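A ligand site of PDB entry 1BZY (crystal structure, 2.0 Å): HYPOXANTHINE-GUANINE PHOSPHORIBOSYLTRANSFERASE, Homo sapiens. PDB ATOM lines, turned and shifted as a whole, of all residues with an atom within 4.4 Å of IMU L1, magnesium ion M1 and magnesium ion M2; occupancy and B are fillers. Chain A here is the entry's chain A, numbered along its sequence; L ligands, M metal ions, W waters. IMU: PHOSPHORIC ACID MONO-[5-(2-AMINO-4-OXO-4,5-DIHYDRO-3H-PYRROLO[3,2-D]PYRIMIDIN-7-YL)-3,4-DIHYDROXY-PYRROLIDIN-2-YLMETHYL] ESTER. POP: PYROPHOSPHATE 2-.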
ATOM      1  N   LEU A  67       6.254   0.439  -5.197  1.00  0.00           N
ATOM      2  CA  LEU A  67       5.015   1.183  -4.977  1.00  0.00           C
ATOM      3  C   LEU A  67       4.661   2.026  -6.207  1.00  0.00           C
ATOM      4  O   LEU A  67       5.550   2.415  -6.969  1.00  0.00           O
ATOM      5  CB  LEU A  67       5.201   2.097  -3.753  1.00  0.00           C
ATOM      6  CG  LEU A  67       4.608   1.794  -2.364  1.00  0.00           C
ATOM      7  CD1 LEU A  67       4.017   0.415  -2.290  1.00  0.00           C
ATOM      8  CD2 LEU A  67       5.687   1.999  -1.321  1.00  0.00           C
ATOM      9  N   GLY A  69       1.838   0.451  -7.431  1.00  0.00           N
ATOM     10  CA  GLY A  69       1.257  -0.672  -8.136  1.00  0.00           C
ATOM     11  C   GLY A  69       1.414  -2.075  -7.599  1.00  0.00           C
ATOM     12  O   GLY A  69       0.465  -2.843  -7.621  1.00  0.00           O
ATOM     13  N   TYR A 104       3.929   6.859 -15.312  1.00  0.00           N
ATOM     14  CA  TYR A 104       2.764   6.825 -16.198  1.00  0.00           C
ATOM     15  C   TYR A 104       1.783   7.969 -16.066  1.00  0.00           C
ATOM     16  O   TYR A 104       1.608   8.527 -14.987  1.00  0.00           O
ATOM     17  CB  TYR A 104       2.001   5.502 -16.021  1.00  0.00           C
ATOM     18  CG  TYR A 104       2.505   4.417 -16.943  1.00  0.00           C
ATOM     19  CD1 TYR A 104       3.791   3.909 -16.802  1.00  0.00           C
ATOM     20  CD2 TYR A 104       1.698   3.916 -17.958  1.00  0.00           C
ATOM     21  CE1 TYR A 104       4.264   2.919 -17.652  1.00  0.00           C
ATOM     22  CE2 TYR A 104       2.173   2.912 -18.809  1.00  0.00           C
ATOM     23  CZ  TYR A 104       3.450   2.423 -18.655  1.00  0.00           C
ATOM     24  OH  TYR A 104       3.931   1.440 -19.486  1.00  0.00           O
ATOM     25  N   SER A 109       3.499   5.699 -20.705  1.00  0.00           N
ATOM     26  CA  SER A 109       4.765   5.815 -20.003  1.00  0.00           C
ATOM     27  C   SER A 109       5.477   7.059 -20.531  1.00  0.00           C
ATOM     28  O   SER A 109       5.756   7.157 -21.729  1.00  0.00           O
ATOM     29  CB  SER A 109       5.643   4.589 -20.255  1.00  0.00           C
ATOM     30  OG  SER A 109       7.000   4.875 -20.014  1.00  0.00           O
ATOM     31  N   GLU A 133       6.984  -6.595  -8.220  1.00  0.00           N
ATOM     32  CA  GLU A 133       6.347  -5.573  -9.037  1.00  0.00           C
ATOM     33  C   GLU A 133       5.009  -6.020  -9.615  1.00  0.00           C
ATOM     34  O   GLU A 133       4.712  -7.213  -9.660  1.00  0.00           O
ATOM     35  CB  GLU A 133       7.313  -5.191 -10.168  1.00  0.00           C
ATOM     36  CG  GLU A 133       6.737  -4.354 -11.280  1.00  0.00           C
ATOM     37  CD  GLU A 133       6.417  -2.945 -10.856  1.00  0.00           C
ATOM     38  OE1 GLU A 133       5.652  -2.785  -9.887  1.00  0.00           O
ATOM     39  OE2 GLU A 133       6.942  -1.990 -11.483  1.00  0.00           O
ATOM     40  N   ASP A 134       4.188  -5.064 -10.050  1.00  0.00           N
ATOM     41  CA  ASP A 134       2.884  -5.376 -10.605  1.00  0.00           C
ATOM     42  C   ASP A 134       2.917  -5.833 -12.050  1.00  0.00           C
ATOM     43  O   ASP A 134       2.325  -6.860 -12.401  1.00  0.00           O
ATOM     44  CB  ASP A 134       1.912  -4.188 -10.452  1.00  0.00           C
ATOM     45  CG  ASP A 134       2.469  -2.882 -11.042  1.00  0.00           C
ATOM     46  OD1 ASP A 134       3.591  -2.885 -11.604  1.00  0.00           O
ATOM     47  OD2 ASP A 134       1.789  -1.849 -10.927  1.00  0.00           O
ATOM     48  N   ILE A 135       3.616  -5.097 -12.902  1.00  0.00           N
ATOM     49  CA  ILE A 135       3.674  -5.473 -14.306  1.00  0.00           C
ATOM     50  C   ILE A 135       4.867  -4.899 -15.067  1.00  0.00           C
ATOM     51  O   ILE A 135       5.344  -3.811 -14.764  1.00  0.00           O
ATOM     52  CB  ILE A 135       2.385  -5.026 -15.030  1.00  0.00           C
ATOM     53  CG1 ILE A 135       2.445  -5.395 -16.504  1.00  0.00           C
ATOM     54  CG2 ILE A 135       2.207  -3.519 -14.877  1.00  0.00           C
ATOM     55  CD1 ILE A 135       1.120  -5.224 -17.229  1.00  0.00           C
ATOM     56  N   ILE A 136       5.353  -5.665 -16.037  1.00  0.00           N
ATOM     57  CA  ILE A 136       6.455  -5.239 -16.894  1.00  0.00           C
ATOM     58  C   ILE A 136       5.786  -4.900 -18.214  1.00  0.00           C
ATOM     59  O   ILE A 136       5.187  -5.770 -18.870  1.00  0.00           O
ATOM     60  CB  ILE A 136       7.483  -6.384 -17.145  1.00  0.00           C
ATOM     61  CG1 ILE A 136       8.076  -6.876 -15.821  1.00  0.00           C
ATOM     62  CG2 ILE A 136       8.571  -5.893 -18.097  1.00  0.00           C
ATOM     63  CD1 ILE A 136       8.868  -5.840 -15.056  1.00  0.00           C
ATOM     64  N   ASP A 137       5.870  -3.636 -18.607  1.00  0.00           N
ATOM     65  CA  ASP A 137       5.263  -3.155 -19.848  1.00  0.00           C
ATOM     66  C   ASP A 137       6.368  -2.845 -20.844  1.00  0.00           C
ATOM     67  O   ASP A 137       6.805  -3.723 -21.580  1.00  0.00           O
ATOM     68  CB  ASP A 137       4.422  -1.903 -19.560  1.00  0.00           C
ATOM     69  CG  ASP A 137       3.400  -1.622 -20.643  1.00  0.00           C
ATOM     70  OD1 ASP A 137       3.740  -1.766 -21.835  1.00  0.00           O
ATOM     71  OD2 ASP A 137       2.247  -1.250 -20.287  1.00  0.00           O
ATOM     72  N   THR A 138       6.853  -1.608 -20.858  1.00  0.00           N
ATOM     73  CA  THR A 138       7.938  -1.245 -21.767  1.00  0.00           C
ATOM     74  C   THR A 138       9.264  -1.748 -21.215  1.00  0.00           C
ATOM     75  O   THR A 138      10.241  -1.879 -21.953  1.00  0.00           O
ATOM     76  CB  THR A 138       8.053   0.282 -21.965  1.00  0.00           C
ATOM     77  OG1 THR A 138       8.480   0.896 -20.739  1.00  0.00           O
ATOM     78  CG2 THR A 138       6.727   0.874 -22.390  1.00  0.00           C
ATOM     79  N   GLY A 139       9.293  -2.018 -19.916  1.00  0.00           N
ATOM     80  CA  GLY A 139      10.498  -2.497 -19.261  1.00  0.00           C
ATOM     81  C   GLY A 139      11.355  -1.380 -18.674  1.00  0.00           C
ATOM     82  O   GLY A 139      12.333  -1.626 -17.978  1.00  0.00           O
ATOM     83  N   LYS A 140      10.961  -0.145 -18.939  1.00  0.00           N
ATOM     84  CA  LYS A 140      11.704   1.017 -18.462  1.00  0.00           C
ATOM     85  C   LYS A 140      11.845   1.090 -16.947  1.00  0.00           C
ATOM     86  O   LYS A 140      12.927   1.353 -16.430  1.00  0.00           O
ATOM     87  CB  LYS A 140      11.036   2.300 -18.963  1.00  0.00           C
ATOM     88  CG  LYS A 140      12.010   3.390 -19.381  1.00  0.00           C
ATOM     89  CD  LYS A 140      12.629   3.080 -20.752  1.00  0.00           C
ATOM     90  CE  LYS A 140      11.584   2.663 -21.772  1.00  0.00           C
ATOM     91  NZ  LYS A 140      11.481   3.646 -22.883  1.00  0.00           N
ATOM     92  N   THR A 141      10.751   0.867 -16.232  1.00  0.00           N
ATOM     93  CA  THR A 141      10.762   0.926 -14.778  1.00  0.00           C
ATOM     94  C   THR A 141      11.696  -0.093 -14.122  1.00  0.00           C
ATOM     95  O   THR A 141      12.520   0.269 -13.291  1.00  0.00           O
ATOM     96  CB  THR A 141       9.351   0.711 -14.213  1.00  0.00           C
ATOM     97  OG1 THR A 141       8.506   1.804 -14.614  1.00  0.00           O
ATOM     98  CG2 THR A 141       9.384   0.652 -12.688  1.00  0.00           C
ATOM     99  N   LYS A 165       3.450  -7.808 -20.008  1.00  0.00           N
ATOM    100  CA  LYS A 165       2.653  -7.451 -21.185  1.00  0.00           C
ATOM    101  C   LYS A 165       3.332  -7.739 -22.513  1.00  0.00           C
ATOM    102  O   LYS A 165       4.505  -7.389 -22.716  1.00  0.00           O
ATOM    103  CB  LYS A 165       2.281  -5.966 -21.133  1.00  0.00           C
ATOM    104  CG  LYS A 165       1.130  -5.592 -22.016  1.00  0.00           C
ATOM    105  CD  LYS A 165       0.907  -4.087 -22.018  1.00  0.00           C
ATOM    106  CE  LYS A 165       0.352  -3.593 -20.688  1.00  0.00           C
ATOM    107  NZ  LYS A 165      -0.353  -2.282 -20.815  1.00  0.00           N
ATOM    108  N   LYS A 185      -2.979  -4.669 -23.442  1.00  0.00           N
ATOM    109  CA  LYS A 185      -4.142  -3.950 -22.952  1.00  0.00           C
ATOM    110  C   LYS A 185      -3.767  -3.275 -21.642  1.00  0.00           C
ATOM    111  O   LYS A 185      -2.958  -3.814 -20.885  1.00  0.00           O
ATOM    112  CB  LYS A 185      -5.308  -4.925 -22.718  1.00  0.00           C
ATOM    113  CG  LYS A 185      -5.862  -5.553 -23.985  1.00  0.00           C
ATOM    114  CD  LYS A 185      -7.348  -5.822 -23.847  1.00  0.00           C
ATOM    115  CE  LYS A 185      -7.926  -6.342 -25.165  1.00  0.00           C
ATOM    116  NZ  LYS A 185      -7.854  -7.825 -25.258  1.00  0.00           N
ATOM    117  N   PHE A 186      -4.341  -2.103 -21.393  1.00  0.00           N
ATOM    118  CA  PHE A 186      -4.055  -1.396 -20.148  1.00  0.00           C
ATOM    119  C   PHE A 186      -5.015  -1.845 -19.062  1.00  0.00           C
ATOM    120  O   PHE A 186      -6.126  -1.320 -18.937  1.00  0.00           O
ATOM    121  CB  PHE A 186      -4.150   0.125 -20.343  1.00  0.00           C
ATOM    122  CG  PHE A 186      -3.458   0.907 -19.251  1.00  0.00           C
ATOM    123  CD1 PHE A 186      -2.090   1.160 -19.320  1.00  0.00           C
ATOM    124  CD2 PHE A 186      -4.167   1.346 -18.142  1.00  0.00           C
ATOM    125  CE1 PHE A 186      -1.439   1.846 -18.298  1.00  0.00           C
ATOM    126  CE2 PHE A 186      -3.523   2.037 -17.109  1.00  0.00           C
ATOM    127  CZ  PHE A 186      -2.148   2.286 -17.189  1.00  0.00           C
ATOM    128  N   VAL A 187      -4.576  -2.810 -18.270  1.00  0.00           N
ATOM    129  CA  VAL A 187      -5.359  -3.361 -17.180  1.00  0.00           C
ATOM    130  C   VAL A 187      -5.324  -2.503 -15.924  1.00  0.00           C
ATOM    131  O   VAL A 187      -4.387  -1.741 -15.697  1.00  0.00           O
ATOM    132  CB  VAL A 187      -4.875  -4.782 -16.830  1.00  0.00           C
ATOM    133  CG1 VAL A 187      -5.142  -5.711 -17.980  1.00  0.00           C
ATOM    134  CG2 VAL A 187      -3.373  -4.764 -16.498  1.00  0.00           C
ATOM    135  N   VAL A 188      -6.354  -2.643 -15.102  1.00  0.00           N
ATOM    136  CA  VAL A 188      -6.462  -1.907 -13.851  1.00  0.00           C
ATOM    137  C   VAL A 188      -6.960  -2.871 -12.772  1.00  0.00           C
ATOM    138  O   VAL A 188      -7.388  -3.979 -13.074  1.00  0.00           O
ATOM    139  CB  VAL A 188      -7.468  -0.758 -13.979  1.00  0.00           C
ATOM    140  CG1 VAL A 188      -6.905   0.314 -14.910  1.00  0.00           C
ATOM    141  CG2 VAL A 188      -8.806  -1.296 -14.502  1.00  0.00           C
ATOM    142  N   LEU A 192      -3.327  -1.890  -9.372  1.00  0.00           N
ATOM    143  CA  LEU A 192      -2.930  -1.276 -10.649  1.00  0.00           C
ATOM    144  C   LEU A 192      -3.976  -0.204 -10.958  1.00  0.00           C
ATOM    145  O   LEU A 192      -5.174  -0.490 -11.021  1.00  0.00           O
ATOM    146  CB  LEU A 192      -2.875  -2.318 -11.768  1.00  0.00           C
ATOM    147  CG  LEU A 192      -1.638  -3.233 -11.857  1.00  0.00           C
ATOM    148  CD1 LEU A 192      -1.877  -4.458 -10.989  1.00  0.00           C
ATOM    149  CD2 LEU A 192      -1.398  -3.670 -13.305  1.00  0.00           C
ATOM    150  N   ASP A 193      -3.502   1.018 -11.154  1.00  0.00           N
ATOM    151  CA  ASP A 193      -4.383   2.166 -11.374  1.00  0.00           C
ATOM    152  C   ASP A 193      -4.383   2.770 -12.778  1.00  0.00           C
ATOM    153  O   ASP A 193      -3.630   2.384 -13.668  1.00  0.00           O
ATOM    154  CB  ASP A 193      -3.992   3.292 -10.425  1.00  0.00           C
ATOM    155  CG  ASP A 193      -2.744   4.023 -10.900  1.00  0.00           C
ATOM    156  OD1 ASP A 193      -1.760   3.332 -11.228  1.00  0.00           O
ATOM    157  OD2 ASP A 193      -2.735   5.278 -10.977  1.00  0.00           O
ATOM    158  N   ARG A 199      -7.407   1.294  -7.922  1.00  0.00           N
ATOM    159  CA  ARG A 199      -6.518   0.541  -7.039  1.00  0.00           C
ATOM    160  C   ARG A 199      -7.382  -0.249  -6.051  1.00  0.00           C
ATOM    161  O   ARG A 199      -7.059  -1.385  -5.688  1.00  0.00           O
ATOM    162  CB  ARG A 199      -5.607   1.500  -6.277  1.00  0.00           C
ATOM    163  CG  ARG A 199      -4.667   2.281  -7.166  1.00  0.00           C
ATOM    164  CD  ARG A 199      -3.313   2.433  -6.508  1.00  0.00           C
ATOM    165  NE  ARG A 199      -2.563   3.543  -7.071  1.00  0.00           N
ATOM    166  CZ  ARG A 199      -1.563   3.391  -7.926  1.00  0.00           C
ATOM    167  NH1 ARG A 199      -1.200   2.169  -8.326  1.00  0.00           N
ATOM    168  NH2 ARG A 199      -0.941   4.468  -8.409  1.00  0.00           N
HETATM  169  P   IMU L   1       7.164   0.150 -17.663  1.00  0.00           P
HETATM  170  C2  IMU L   1      -1.607  -0.357 -15.076  1.00  0.00           C
HETATM  171  O1P IMU L   1       7.562  -1.270 -17.735  1.00  0.00           O
HETATM  172  O2P IMU L   1       8.230   1.053 -17.205  1.00  0.00           O
HETATM  173  O3P IMU L   1       6.568   0.573 -18.960  1.00  0.00           O
HETATM  174  O5' IMU L   1       5.944   0.244 -16.745  1.00  0.00           O
HETATM  175  C5' IMU L   1       5.658  -0.545 -15.609  1.00  0.00           C
HETATM  176  C4' IMU L   1       5.150   0.370 -14.575  1.00  0.00           C
HETATM  177  N4' IMU L   1       4.059   1.140 -15.078  1.00  0.00           N
HETATM  178  C3' IMU L   1       4.710  -0.424 -13.403  1.00  0.00           C
HETATM  179  O3' IMU L   1       5.325   0.148 -12.251  1.00  0.00           O
HETATM  180  C2' IMU L   1       3.217  -0.279 -13.442  1.00  0.00           C
HETATM  181  O2' IMU L   1       2.682   0.079 -12.174  1.00  0.00           O
HETATM  182  C1' IMU L   1       2.811   0.784 -14.507  1.00  0.00           C
HETATM  183  C9  IMU L   1       1.991   0.085 -15.603  1.00  0.00           C
HETATM  184  C8  IMU L   1       2.496  -0.429 -16.815  1.00  0.00           C
HETATM  185  N7  IMU L   1       1.621  -0.995 -17.599  1.00  0.00           N
HETATM  186  C5  IMU L   1       0.418  -0.885 -16.886  1.00  0.00           C
HETATM  187  C6  IMU L   1      -0.898  -1.347 -17.255  1.00  0.00           C
HETATM  188  O6  IMU L   1      -1.210  -1.943 -18.276  1.00  0.00           O
HETATM  189  N1  IMU L   1      -1.870  -1.041 -16.283  1.00  0.00           N
HETATM  190  N2  IMU L   1      -2.641  -0.136 -14.252  1.00  0.00           N
HETATM  191  N3  IMU L   1      -0.353   0.073 -14.729  1.00  0.00           N
HETATM  192  C4  IMU L   1       0.621  -0.221 -15.670  1.00  0.00           C
HETATM  193  P1  POP L   2       2.123   3.468  -9.689  1.00  0.00           P
HETATM  194  O1  POP L   2       2.234   4.277  -8.438  1.00  0.00           O
HETATM  195  O2  POP L   2       2.774   2.013  -9.541  1.00  0.00           O
HETATM  196  O3  POP L   2       0.700   3.326 -10.061  1.00  0.00           O
HETATM  197  O   POP L   2       2.979   4.187 -10.781  1.00  0.00           O
HETATM  198  P2  POP L   2       3.311   3.949 -12.303  1.00  0.00           P
HETATM  199  O4  POP L   2       2.083   3.581 -13.016  1.00  0.00           O
HETATM  200  O5  POP L   2       4.346   2.912 -12.457  1.00  0.00           O
HETATM  201  O6  POP L   2       3.848   5.370 -12.771  1.00  0.00           O
HETATM  202 MG    MG M   1       4.195   1.059 -10.739  1.00  0.00          MG
HETATM  203 MG    MG M   2       0.144   3.423 -12.187  1.00  0.00          MG
HETATM  204  O   HOH W   1       9.460  -2.164 -16.043  1.00  0.00           O
HETATM  205  O   HOH W   2       7.842   3.791 -17.652  1.00  0.00           O
HETATM  206  O   HOH W   3       5.880   2.128  -9.875  1.00  0.00           O
HETATM  207  O   HOH W   4      -0.851   3.259 -14.013  1.00  0.00           O
HETATM  208  O   HOH W   5      -0.186   5.675 -12.267  1.00  0.00           O
HETATM  209  O   HOH W   6      -0.035   1.219 -12.314  1.00  0.00           O
HETATM  210  O   HOH W   7       4.386  -0.460  -9.138  1.00  0.00           O
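The backbone carbonyl oxygen (O) of Asp 193 sits at hydrogen-bond distance from a nitrogen (N2) of IMU L1 (2.8 Å).
The side-chain carboxylate (OD2) of Asp 134 sits close to an oxygen (O2') of IMU L1 (2.5 Å).
An oxygen (O3P) of IMU L1 is in hydrogen-bond range of the backbone NH (N) of Thr 138 (2.9 Å).
The side-chain hydroxyl of Thr 138 lies within hydrogen-bond range of an oxygen (O3P) of IMU L1 (2.6 Å).
The backbone NH (N) of Val 187 lies within hydrogen-bond range of an oxygen (O6) of IMU L1 (3.5 Å).
The backbone carbonyl oxygen of Val 187 sits at hydrogen-bond distance from a nitrogen (N1) of IMU L1 (2.7 Å).
The side-chain amino group of Lys 165 is in hydrogen-bond range of an oxygen (O6) of IMU L1 (2.7 Å).
An oxygen (O2P) of IMU L1 sits at hydrogen-bond distance from the backbone NH (N) of Thr 141 (2.7 Å).
An oxygen (O2P) of IMU L1 lies within hydrogen-bond range of the side-chain hydroxyl (OG1) of Thr 141, 2.7 Å away.
N of Asp 137 lies within hydrogen-bond range of O1P of IMU L1 (3.0 Å).
A nitrogen (N7) of IMU L1 lies within hydrogen-bond range of the side-chain carboxylate (OD2) of Asp 137, at 2.8 Å.
OE2 of Glu 133 sits close to O3' of IMU L1, at 2.8 Å.
The side-chain hydroxyl (OH) of Tyr 104 sits at hydrogen-bond distance from an oxygen (O3P) of IMU L1 (2.8 Å).
An oxygen (O1P) of IMU L1 is in hydrogen-bond range of the backbone NH (N) of Gly 139 (2.9 Å).
The backbone NH of Lys 140 lies within hydrogen-bond range of an oxygen (O2P) of IMU L1, at 3.4 Å.
An oxygen (O6) of POP L2 lies within hydrogen-bond range of the backbone NH of Tyr 104 (2.9 Å).
The guanidinium group of Arg 199 lies within salt-bridge range of an oxygen (O1) of POP L2, 3.2 Å away.
The backbone NH of Gly 69 lies close to an oxygen (O2) of POP L2, at 2.8 Å.
The guanidinium group (NH2) of Arg 199 lies within salt-bridge range of the side-chain carboxylate (OD2) of Asp 193, at 3.2 Å.
OD1 of Asp 134 lies close to OE1 of Glu 133, 2.7 Å away.
The side-chain hydroxyl of Thr 138 is in hydrogen-bond range of the backbone NH of Lys 140 (3.2 Å).
The side-chain amino group (NZ) of Lys 165 lies within salt-bridge range of the side-chain carboxylate (OD2) of Asp 137 (2.8 Å).
The backbone carbonyl oxygen (O) of Lys 185 sits at hydrogen-bond distance from the side-chain amino group (NZ) of Lys 165, at 3.0 Å.
N of Lys 165 sits at hydrogen-bond distance from O of Ile 136, at 2.9 Å.
OD2 of Asp 137 lies within hydrogen-bond range of OH of Tyr 104 (3.3 Å).
Ile 135 touches IMU L1.
Lys 185 touches IMU L1.
CD1 of Phe 186 touches O6 of IMU L1, 3.4 Å away.
Leu 192 touches IMU L1 (CB to N2, 3.3 Å).
Hydrophobic or aromatic side chains within 4 Å of IMU L1: Tyr 104, Ile 135, Phe 186, Val 187 and Leu 192.
Within 4 Å of IMU L1: Tyr 104, Glu 133, Asp 134, Ile 135, Asp 137, Thr 138, Gly 139, Lys 140, Thr 141, Lys 165, Lys 185, Phe 186, Val 187, Leu 192 and Asp 193.
The nearest printed residue that does not touch IMU L1 is Ile 136 (4.1 Å).
Asp 134 touches magnesium ion M1 (OD2 to MG, 3.8 Å).
Of the 21 residues printed, 1 comes within 4 Å of magnesium ion M1.
One residue has an atom within 4 Å of magnesium ion M2: Asp 193.
O2 of POP L2 is bound to magnesium ion M1 (2.1 Å).
Magnesium ion M1 is bound by an oxygen (O3') of IMU L1 (2.1 Å).
Magnesium ion M1 is bound by water W3 (2.2 Å).
Magnesium ion M1 is bound by water W7, at 2.2 Å.
An oxygen (O2') of IMU L1 binds magnesium ion M1.
Magnesium ion M1 is bound by an oxygen (O5) of POP L2 (2.5 Å).
Magnesium ion M1 has six donor atoms within binding distance.
Magnesium ion M2 is bound by water W4, O4 of POP L2, OD1 of Asp 193, O3 of POP L2, water W6 and water W5.
Magnesium ion M2 has six donor atoms within binding distance.
Water W7 lies within hydrogen-bond range of the side-chain carboxylate (OE1) of Glu 133, the backbone NH (N) of Gly 69 and the side-chain carboxylate (OD2) of Asp 134.
Water W4 bridges the backbone carbonyl oxygen (O) of Asp 193 (2.9 Å) and a nitrogen (N3) of IMU L1 (3.3 Å).
Water W1 lies within hydrogen-bond range of an oxygen (O1P) of IMU L1 (2.7 Å) and the backbone NH of Thr 141 (3.3 Å).
Water W2 bridges the side-chain hydroxyl (OG) of Ser 109 and an oxygen (O2P) of IMU L1.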
